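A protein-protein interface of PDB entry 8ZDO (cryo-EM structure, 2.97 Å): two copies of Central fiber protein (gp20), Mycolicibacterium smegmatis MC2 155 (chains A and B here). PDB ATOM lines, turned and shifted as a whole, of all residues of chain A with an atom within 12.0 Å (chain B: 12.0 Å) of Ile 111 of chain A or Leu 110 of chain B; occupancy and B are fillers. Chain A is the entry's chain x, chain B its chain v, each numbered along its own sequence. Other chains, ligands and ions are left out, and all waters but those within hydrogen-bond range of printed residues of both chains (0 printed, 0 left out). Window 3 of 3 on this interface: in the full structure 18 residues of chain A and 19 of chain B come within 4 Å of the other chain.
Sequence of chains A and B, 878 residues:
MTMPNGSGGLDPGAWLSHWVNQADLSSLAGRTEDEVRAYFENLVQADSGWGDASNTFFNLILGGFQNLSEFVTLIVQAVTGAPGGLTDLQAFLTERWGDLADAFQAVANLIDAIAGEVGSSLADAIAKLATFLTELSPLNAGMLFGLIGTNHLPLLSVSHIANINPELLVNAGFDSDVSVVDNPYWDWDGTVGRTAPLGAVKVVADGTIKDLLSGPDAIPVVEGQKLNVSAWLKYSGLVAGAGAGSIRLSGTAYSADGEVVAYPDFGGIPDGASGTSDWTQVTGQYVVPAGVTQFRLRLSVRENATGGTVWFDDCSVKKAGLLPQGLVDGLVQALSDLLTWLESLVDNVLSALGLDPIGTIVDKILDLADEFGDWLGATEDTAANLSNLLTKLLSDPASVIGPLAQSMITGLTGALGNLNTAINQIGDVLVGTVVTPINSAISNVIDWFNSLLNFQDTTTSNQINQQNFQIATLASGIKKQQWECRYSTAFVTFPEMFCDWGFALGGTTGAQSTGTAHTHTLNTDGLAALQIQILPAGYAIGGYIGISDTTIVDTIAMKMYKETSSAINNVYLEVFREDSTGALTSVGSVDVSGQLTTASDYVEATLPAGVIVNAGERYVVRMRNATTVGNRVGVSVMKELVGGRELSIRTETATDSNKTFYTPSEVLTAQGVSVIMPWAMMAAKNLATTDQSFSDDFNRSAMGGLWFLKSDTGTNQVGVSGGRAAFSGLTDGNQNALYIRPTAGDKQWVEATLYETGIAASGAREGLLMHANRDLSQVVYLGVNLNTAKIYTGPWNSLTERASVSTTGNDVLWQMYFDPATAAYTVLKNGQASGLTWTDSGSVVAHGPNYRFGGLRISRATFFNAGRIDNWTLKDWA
Printed residues of chain A that touch a printed residue of chain B: Phe 104, Val 107, Leu 110, Ile 111 and Ile 114.
Hydrophobic or aromatic side chains of chain A that line the printed part of chain B: Phe 104, Val 107, Leu 110, Ile 111 and Ile 114.
Hydrophobic or aromatic side chains of chain B within 4 Å of the printed part of chain A: Ala 103, Val 107, Leu 110 and Ile 114.
Among the printed residues, no Asp or Glu carboxylate lies within 4 Å of a Lys or Arg side-chain nitrogen of the other chain.
Of the printed residues of chain B, Phe 104 of chain A touches Ala 103 (3.5 Å).
Ala 108 of chain A touches none of the printed residues of chain B.
Of chain B, only Leu 110 (3.7 Å) comes within 4 Å of Leu 110 of chain A.
Ile 111 of chain A touches just one residue of chain B: Leu 110.
No residue of chain B comes within 4 Å of Ala 113 of chain A.
Ile 114 of chain A touches just one residue of chain B: Ile 114 (3.7 Å).
No residue of chain B comes within 4 Å of Ala 115 of chain A.
Of the printed residues of chain A, Ala 103 of chain B touches Phe 104 (3.5 Å).
No residue of chain A comes within 4 Å of Ala 106 of chain B.
No residue of chain A comes within 4 Å of Ala 108 of chain B.
No residue of chain A comes within 4 Å of Asn 109 of chain B.
Of chain A, only Leu 110 (3.7 Å) and Ile 111 (3.7 Å) come within 4 Å of Leu 110 of chain B.
Asp 112 of chain B touches none of the printed residues of chain A.
No residue of chain A comes within 4 Å of Ala 113 of chain B.
Ile 114 of chain B touches just one residue of chain A: Ile 114.
Ala 115 of chain B touches none of the printed residues of chain A.
Among the printed residues, merely in contact across the chains: Phe 104 of chain A with Ala 103 of chain B, Val 107 of chain A with Val 107 of chain B, Leu 110 of chain A with Leu 110 of chain B, Ile 111 of chain A with Leu 110 of chain B and Ile 114 of chain A with Ile 114 of chain B.
Phe 104 of chain A touches Ala 103 of chain B, but with the chains exchanged Ala 103 of chain A does not touch Phe 104 of chain B (7.9 Å).
Val 107 of chain B touches its own counterpart, Val 107 of chain A.
Leu 110 of chain B touches its own counterpart, Leu 110 of chain A.
Ile 111 of chain A touches Leu 110 of chain B, but with the chains exchanged Leu 110 of chain A does not touch Ile 111 of chain B (8.4 Å).
Of the 5 pairs that touch across the chains among the printed residues, 3 have their exchanged pair printed and touching as well.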
ATOM      1  N   ASP A 102     -18.380   6.385 -17.454  1.00  0.00           N
ATOM      2  CA  ASP A 102     -18.436   6.326 -15.997  1.00  0.00           C
ATOM      3  C   ASP A 102     -17.223   7.002 -15.371  1.00  0.00           C
ATOM      4  O   ASP A 102     -17.349   7.713 -14.369  1.00  0.00           O
ATOM      5  CB  ASP A 102     -18.544   4.874 -15.533  1.00  0.00           C
ATOM      6  CG  ASP A 102     -19.888   4.258 -15.861  1.00  0.00           C
ATOM      7  OD1 ASP A 102     -20.887   5.005 -15.914  1.00  0.00           O
ATOM      8  OD2 ASP A 102     -19.947   3.025 -16.062  1.00  0.00           O
ATOM      9  N   ALA A 103     -16.038   6.795 -15.948  1.00  0.00           N
ATOM     10  CA  ALA A 103     -14.840   7.447 -15.424  1.00  0.00           C
ATOM     11  C   ALA A 103     -14.907   8.963 -15.589  1.00  0.00           C
ATOM     12  O   ALA A 103     -14.496   9.712 -14.693  1.00  0.00           O
ATOM     13  CB  ALA A 103     -13.597   6.888 -16.111  1.00  0.00           C
ATOM     14  N   PHE A 104     -15.408   9.437 -16.732  1.00  0.00           N
ATOM     15  CA  PHE A 104     -15.526  10.879 -16.932  1.00  0.00           C
ATOM     16  C   PHE A 104     -16.536  11.484 -15.963  1.00  0.00           C
ATOM     17  O   PHE A 104     -16.312  12.572 -15.414  1.00  0.00           O
ATOM     18  CB  PHE A 104     -15.914  11.184 -18.381  1.00  0.00           C
ATOM     19  CG  PHE A 104     -14.818  10.916 -19.378  1.00  0.00           C
ATOM     20  CD1 PHE A 104     -13.620  10.338 -18.985  1.00  0.00           C
ATOM     21  CD2 PHE A 104     -14.985  11.250 -20.712  1.00  0.00           C
ATOM     22  CE1 PHE A 104     -12.618  10.091 -19.901  1.00  0.00           C
ATOM     23  CE2 PHE A 104     -13.983  11.011 -21.633  1.00  0.00           C
ATOM     24  CZ  PHE A 104     -12.799  10.429 -21.226  1.00  0.00           C
ATOM     25  N   GLN A 105     -17.651  10.788 -15.731  1.00  0.00           N
ATOM     26  CA  GLN A 105     -18.604  11.246 -14.728  1.00  0.00           C
ATOM     27  C   GLN A 105     -18.004  11.193 -13.329  1.00  0.00           C
ATOM     28  O   GLN A 105     -18.358  12.012 -12.478  1.00  0.00           O
ATOM     29  CB  GLN A 105     -19.885  10.416 -14.797  1.00  0.00           C
ATOM     30  CG  GLN A 105     -20.663  10.598 -16.092  1.00  0.00           C
ATOM     31  CD  GLN A 105     -21.009  12.049 -16.370  1.00  0.00           C
ATOM     32  OE1 GLN A 105     -21.418  12.786 -15.473  1.00  0.00           O
ATOM     33  NE2 GLN A 105     -20.840  12.468 -17.619  1.00  0.00           N
ATOM     34  N   ALA A 106     -17.097  10.248 -13.074  1.00  0.00           N
ATOM     35  CA  ALA A 106     -16.388  10.222 -11.798  1.00  0.00           C
ATOM     36  C   ALA A 106     -15.487  11.441 -11.643  1.00  0.00           C
ATOM     37  O   ALA A 106     -15.367  11.995 -10.547  1.00  0.00           O
ATOM     38  CB  ALA A 106     -15.577   8.933 -11.672  1.00  0.00           C
ATOM     39  N   VAL A 107     -14.828  11.857 -12.725  1.00  0.00           N
ATOM     40  CA  VAL A 107     -14.030  13.083 -12.679  1.00  0.00           C
ATOM     41  C   VAL A 107     -14.920  14.288 -12.396  1.00  0.00           C
ATOM     42  O   VAL A 107     -14.580  15.165 -11.587  1.00  0.00           O
ATOM     43  CB  VAL A 107     -13.243  13.262 -13.992  1.00  0.00           C
ATOM     44  CG1 VAL A 107     -12.418  14.540 -13.948  1.00  0.00           C
ATOM     45  CG2 VAL A 107     -12.353  12.061 -14.244  1.00  0.00           C
ATOM     46  N   ALA A 108     -16.076  14.349 -13.063  1.00  0.00           N
ATOM     47  CA  ALA A 108     -17.023  15.430 -12.804  1.00  0.00           C
ATOM     48  C   ALA A 108     -17.492  15.412 -11.353  1.00  0.00           C
ATOM     49  O   ALA A 108     -17.635  16.467 -10.723  1.00  0.00           O
ATOM     50  CB  ALA A 108     -18.213  15.328 -13.756  1.00  0.00           C
ATOM     51  N   ASN A 109     -17.736  14.219 -10.806  1.00  0.00           N
ATOM     52  CA  ASN A 109     -18.138  14.095  -9.410  1.00  0.00           C
ATOM     53  C   ASN A 109     -17.020  14.505  -8.462  1.00  0.00           C
ATOM     54  O   ASN A 109     -17.295  15.052  -7.394  1.00  0.00           O
ATOM     55  CB  ASN A 109     -18.588  12.664  -9.116  1.00  0.00           C
ATOM     56  CG  ASN A 109     -19.863  12.293  -9.848  1.00  0.00           C
ATOM     57  OD1 ASN A 109     -20.533  13.149 -10.425  1.00  0.00           O
ATOM     58  ND2 ASN A 109     -20.204  11.010  -9.828  1.00  0.00           N
ATOM     59  N   LEU A 110     -15.764  14.238  -8.823  1.00  0.00           N
ATOM     60  CA  LEU A 110     -14.647  14.746  -8.032  1.00  0.00           C
ATOM     61  C   LEU A 110     -14.634  16.266  -8.014  1.00  0.00           C
ATOM     62  O   LEU A 110     -14.416  16.882  -6.962  1.00  0.00           O
ATOM     63  CB  LEU A 110     -13.323  14.213  -8.580  1.00  0.00           C
ATOM     64  CG  LEU A 110     -13.012  12.745  -8.317  1.00  0.00           C
ATOM     65  CD1 LEU A 110     -11.793  12.307  -9.106  1.00  0.00           C
ATOM     66  CD2 LEU A 110     -12.764  12.580  -6.831  1.00  0.00           C
ATOM     67  N   ILE A 111     -14.859  16.888  -9.172  1.00  0.00           N
ATOM     68  CA  ILE A 111     -14.916  18.348  -9.225  1.00  0.00           C
ATOM     69  C   ILE A 111     -16.054  18.862  -8.347  1.00  0.00           C
ATOM     70  O   ILE A 111     -15.883  19.796  -7.553  1.00  0.00           O
ATOM     71  CB  ILE A 111     -15.057  18.829 -10.680  1.00  0.00           C
ATOM     72  CG1 ILE A 111     -13.695  18.820 -11.375  1.00  0.00           C
ATOM     73  CG2 ILE A 111     -15.677  20.220 -10.732  1.00  0.00           C
ATOM     74  CD1 ILE A 111     -12.732  19.861 -10.846  1.00  0.00           C
ATOM     75  N   ASP A 112     -17.225  18.234  -8.456  1.00  0.00           N
ATOM     76  CA  ASP A 112     -18.375  18.660  -7.663  1.00  0.00           C
ATOM     77  C   ASP A 112     -18.130  18.462  -6.169  1.00  0.00           C
ATOM     78  O   ASP A 112     -18.530  19.297  -5.352  1.00  0.00           O
ATOM     79  CB  ASP A 112     -19.625  17.903  -8.111  1.00  0.00           C
ATOM     80  CG  ASP A 112     -19.895  18.056  -9.594  1.00  0.00           C
ATOM     81  OD1 ASP A 112     -19.335  18.989 -10.207  1.00  0.00           O
ATOM     82  OD2 ASP A 112     -20.663  17.241 -10.148  1.00  0.00           O
ATOM     83  N   ALA A 113     -17.478  17.359  -5.794  1.00  0.00           N
ATOM     84  CA  ALA A 113     -17.224  17.077  -4.385  1.00  0.00           C
ATOM     85  C   ALA A 113     -16.215  18.051  -3.797  1.00  0.00           C
ATOM     86  O   ALA A 113     -16.414  18.560  -2.688  1.00  0.00           O
ATOM     87  CB  ALA A 113     -16.742  15.636  -4.219  1.00  0.00           C
ATOM     88  N   ILE A 114     -15.123  18.321  -4.517  1.00  0.00           N
ATOM     89  CA  ILE A 114     -14.173  19.315  -4.039  1.00  0.00           C
ATOM     90  C   ILE A 114     -14.794  20.706  -4.044  1.00  0.00           C
ATOM     91  O   ILE A 114     -14.335  21.589  -3.310  1.00  0.00           O
ATOM     92  CB  ILE A 114     -12.871  19.275  -4.864  1.00  0.00           C
ATOM     93  CG1 ILE A 114     -11.737  19.967  -4.102  1.00  0.00           C
ATOM     94  CG2 ILE A 114     -13.061  19.922  -6.221  1.00  0.00           C
ATOM     95  CD1 ILE A 114     -11.474  19.380  -2.733  1.00  0.00           C
ATOM     96  N   ALA A 115     -15.839  20.922  -4.848  1.00  0.00           N
ATOM     97  CA  ALA A 115     -16.605  22.157  -4.729  1.00  0.00           C
ATOM     98  C   ALA A 115     -17.492  22.151  -3.492  1.00  0.00           C
ATOM     99  O   ALA A 115     -17.749  23.211  -2.909  1.00  0.00           O
ATOM    100  CB  ALA A 115     -17.444  22.378  -5.986  1.00  0.00           C
ATOM    101  N   ALA B 101      -8.666  13.522 -24.456  1.00  0.00           N
ATOM    102  CA  ALA B 101      -7.581  14.430 -24.097  1.00  0.00           C
ATOM    103  C   ALA B 101      -8.088  15.562 -23.213  1.00  0.00           C
ATOM    104  O   ALA B 101      -7.403  15.981 -22.273  1.00  0.00           O
ATOM    105  CB  ALA B 101      -6.919  14.984 -25.358  1.00  0.00           C
ATOM    106  N   ASP B 102      -9.287  16.070 -23.504  1.00  0.00           N
ATOM    107  CA  ASP B 102      -9.880  17.102 -22.659  1.00  0.00           C
ATOM    108  C   ASP B 102     -10.125  16.581 -21.248  1.00  0.00           C
ATOM    109  O   ASP B 102      -9.899  17.297 -20.268  1.00  0.00           O
ATOM    110  CB  ASP B 102     -11.181  17.605 -23.282  1.00  0.00           C
ATOM    111  CG  ASP B 102     -10.955  18.341 -24.587  1.00  0.00           C
ATOM    112  OD1 ASP B 102      -9.805  18.757 -24.843  1.00  0.00           O
ATOM    113  OD2 ASP B 102     -11.925  18.500 -25.357  1.00  0.00           O
ATOM    114  N   ALA B 103     -10.586  15.336 -21.124  1.00  0.00           N
ATOM    115  CA  ALA B 103     -10.790  14.752 -19.801  1.00  0.00           C
ATOM    116  C   ALA B 103      -9.468  14.560 -19.065  1.00  0.00           C
ATOM    117  O   ALA B 103      -9.388  14.781 -17.850  1.00  0.00           O
ATOM    118  CB  ALA B 103     -11.535  13.425 -19.922  1.00  0.00           C
ATOM    119  N   PHE B 104      -8.423  14.137 -19.780  1.00  0.00           N
ATOM    120  CA  PHE B 104      -7.112  13.989 -19.151  1.00  0.00           C
ATOM    121  C   PHE B 104      -6.591  15.334 -18.659  1.00  0.00           C
ATOM    122  O   PHE B 104      -6.048  15.438 -17.549  1.00  0.00           O
ATOM    123  CB  PHE B 104      -6.118  13.359 -20.130  1.00  0.00           C
ATOM    124  CG  PHE B 104      -6.575  12.047 -20.716  1.00  0.00           C
ATOM    125  CD1 PHE B 104      -7.515  11.261 -20.069  1.00  0.00           C
ATOM    126  CD2 PHE B 104      -6.055  11.604 -21.922  1.00  0.00           C
ATOM    127  CE1 PHE B 104      -7.932  10.061 -20.618  1.00  0.00           C
ATOM    128  CE2 PHE B 104      -6.466  10.404 -22.472  1.00  0.00           C
ATOM    129  CZ  PHE B 104      -7.405   9.632 -21.818  1.00  0.00           C
ATOM    130  N   GLN B 105      -6.752  16.381 -19.471  1.00  0.00           N
ATOM    131  CA  GLN B 105      -6.348  17.715 -19.042  1.00  0.00           C
ATOM    132  C   GLN B 105      -7.213  18.221 -17.896  1.00  0.00           C
ATOM    133  O   GLN B 105      -6.731  18.977 -17.053  1.00  0.00           O
ATOM    134  CB  GLN B 105      -6.392  18.687 -20.221  1.00  0.00           C
ATOM    135  CG  GLN B 105      -5.445  18.321 -21.353  1.00  0.00           C
ATOM    136  CD  GLN B 105      -4.040  18.019 -20.864  1.00  0.00           C
ATOM    137  OE1 GLN B 105      -3.444  18.803 -20.125  1.00  0.00           O
ATOM    138  NE2 GLN B 105      -3.507  16.874 -21.272  1.00  0.00           N
ATOM    139  N   ALA B 106      -8.484  17.815 -17.845  1.00  0.00           N
ATOM    140  CA  ALA B 106      -9.324  18.155 -16.701  1.00  0.00           C
ATOM    141  C   ALA B 106      -8.815  17.491 -15.430  1.00  0.00           C
ATOM    142  O   ALA B 106      -8.824  18.102 -14.357  1.00  0.00           O
ATOM    143  CB  ALA B 106     -10.773  17.753 -16.974  1.00  0.00           C
ATOM    144  N   VAL B 107      -8.374  16.237 -15.530  1.00  0.00           N
ATOM    145  CA  VAL B 107      -7.780  15.559 -14.378  1.00  0.00           C
ATOM    146  C   VAL B 107      -6.507  16.276 -13.938  1.00  0.00           C
ATOM    147  O   VAL B 107      -6.262  16.468 -12.739  1.00  0.00           O
ATOM    148  CB  VAL B 107      -7.517  14.078 -14.706  1.00  0.00           C
ATOM    149  CG1 VAL B 107      -6.747  13.408 -13.579  1.00  0.00           C
ATOM    150  CG2 VAL B 107      -8.830  13.355 -14.963  1.00  0.00           C
ATOM    151  N   ALA B 108      -5.678  16.684 -14.903  1.00  0.00           N
ATOM    152  CA  ALA B 108      -4.472  17.440 -14.571  1.00  0.00           C
ATOM    153  C   ALA B 108      -4.815  18.774 -13.908  1.00  0.00           C
ATOM    154  O   ALA B 108      -4.141  19.203 -12.964  1.00  0.00           O
ATOM    155  CB  ALA B 108      -3.629  17.662 -15.825  1.00  0.00           C
ATOM    156  N   ASN B 109      -5.856  19.448 -14.397  1.00  0.00           N
ATOM    157  CA  ASN B 109      -6.295  20.693 -13.779  1.00  0.00           C
ATOM    158  C   ASN B 109      -6.847  20.459 -12.380  1.00  0.00           C
ATOM    159  O   ASN B 109      -6.737  21.336 -11.519  1.00  0.00           O
ATOM    160  CB  ASN B 109      -7.343  21.376 -14.655  1.00  0.00           C
ATOM    161  CG  ASN B 109      -6.790  21.801 -15.999  1.00  0.00           C
ATOM    162  OD1 ASN B 109      -5.575  21.868 -16.192  1.00  0.00           O
ATOM    163  ND2 ASN B 109      -7.681  22.092 -16.940  1.00  0.00           N
ATOM    164  N   LEU B 110      -7.456  19.299 -12.140  1.00  0.00           N
ATOM    165  CA  LEU B 110      -7.881  18.962 -10.785  1.00  0.00           C
ATOM    166  C   LEU B 110      -6.670  18.755  -9.880  1.00  0.00           C
ATOM    167  O   LEU B 110      -6.685  19.159  -8.712  1.00  0.00           O
ATOM    168  CB  LEU B 110      -8.778  17.726 -10.812  1.00  0.00           C
ATOM    169  CG  LEU B 110      -9.664  17.448  -9.592  1.00  0.00           C
ATOM    170  CD1 LEU B 110     -10.929  16.716 -10.016  1.00  0.00           C
ATOM    171  CD2 LEU B 110      -8.930  16.658  -8.530  1.00  0.00           C
ATOM    172  N   ILE B 111      -5.609  18.139 -10.413  1.00  0.00           N
ATOM    173  CA  ILE B 111      -4.332  18.088  -9.700  1.00  0.00           C
ATOM    174  C   ILE B 111      -3.881  19.491  -9.330  1.00  0.00           C
ATOM    175  O   ILE B 111      -3.493  19.767  -8.187  1.00  0.00           O
ATOM    176  CB  ILE B 111      -3.260  17.386 -10.553  1.00  0.00           C
ATOM    177  CG1 ILE B 111      -3.673  15.962 -10.897  1.00  0.00           C
ATOM    178  CG2 ILE B 111      -1.911  17.401  -9.845  1.00  0.00           C
ATOM    179  CD1 ILE B 111      -3.851  15.117  -9.684  1.00  0.00           C
ATOM    180  N   ASP B 112      -3.917  20.397 -10.304  1.00  0.00           N
ATOM    181  CA  ASP B 112      -3.433  21.755 -10.086  1.00  0.00           C
ATOM    182  C   ASP B 112      -4.286  22.495  -9.061  1.00  0.00           C
ATOM    183  O   ASP B 112      -3.762  23.255  -8.240  1.00  0.00           O
ATOM    184  CB  ASP B 112      -3.396  22.500 -11.418  1.00  0.00           C
ATOM    185  CG  ASP B 112      -2.587  21.765 -12.466  1.00  0.00           C
ATOM    186  OD1 ASP B 112      -1.793  20.877 -12.087  1.00  0.00           O
ATOM    187  OD2 ASP B 112      -2.743  22.072 -13.667  1.00  0.00           O
ATOM    188  N   ALA B 113      -5.604  22.288  -9.098  1.00  0.00           N
ATOM    189  CA  ALA B 113      -6.493  22.923  -8.131  1.00  0.00           C
ATOM    190  C   ALA B 113      -6.259  22.386  -6.726  1.00  0.00           C
ATOM    191  O   ALA B 113      -6.257  23.155  -5.755  1.00  0.00           O
ATOM    192  CB  ALA B 113      -7.949  22.717  -8.548  1.00  0.00           C
ATOM    193  N   ILE B 114      -6.071  21.070  -6.591  1.00  0.00           N
ATOM    194  CA  ILE B 114      -5.775  20.494  -5.282  1.00  0.00           C
ATOM    195  C   ILE B 114      -4.449  21.029  -4.759  1.00  0.00           C
ATOM    196  O   ILE B 114      -4.295  21.291  -3.559  1.00  0.00           O
ATOM    197  CB  ILE B 114      -5.783  18.956  -5.357  1.00  0.00           C
ATOM    198  CG1 ILE B 114      -7.191  18.445  -5.664  1.00  0.00           C
ATOM    199  CG2 ILE B 114      -5.286  18.346  -4.056  1.00  0.00           C
ATOM    200  CD1 ILE B 114      -8.264  19.063  -4.798  1.00  0.00           C
ATOM    201  N   ALA B 115      -3.475  21.212  -5.652  1.00  0.00           N
ATOM    202  CA  ALA B 115      -2.191  21.779  -5.265  1.00  0.00           C
ATOM    203  C   ALA B 115      -2.224  23.297  -5.130  1.00  0.00           C
ATOM    204  O   ALA B 115      -1.216  23.888  -4.731  1.00  0.00           O
ATOM    205  CB  ALA B 115      -1.116  21.373  -6.272  1.00  0.00           C
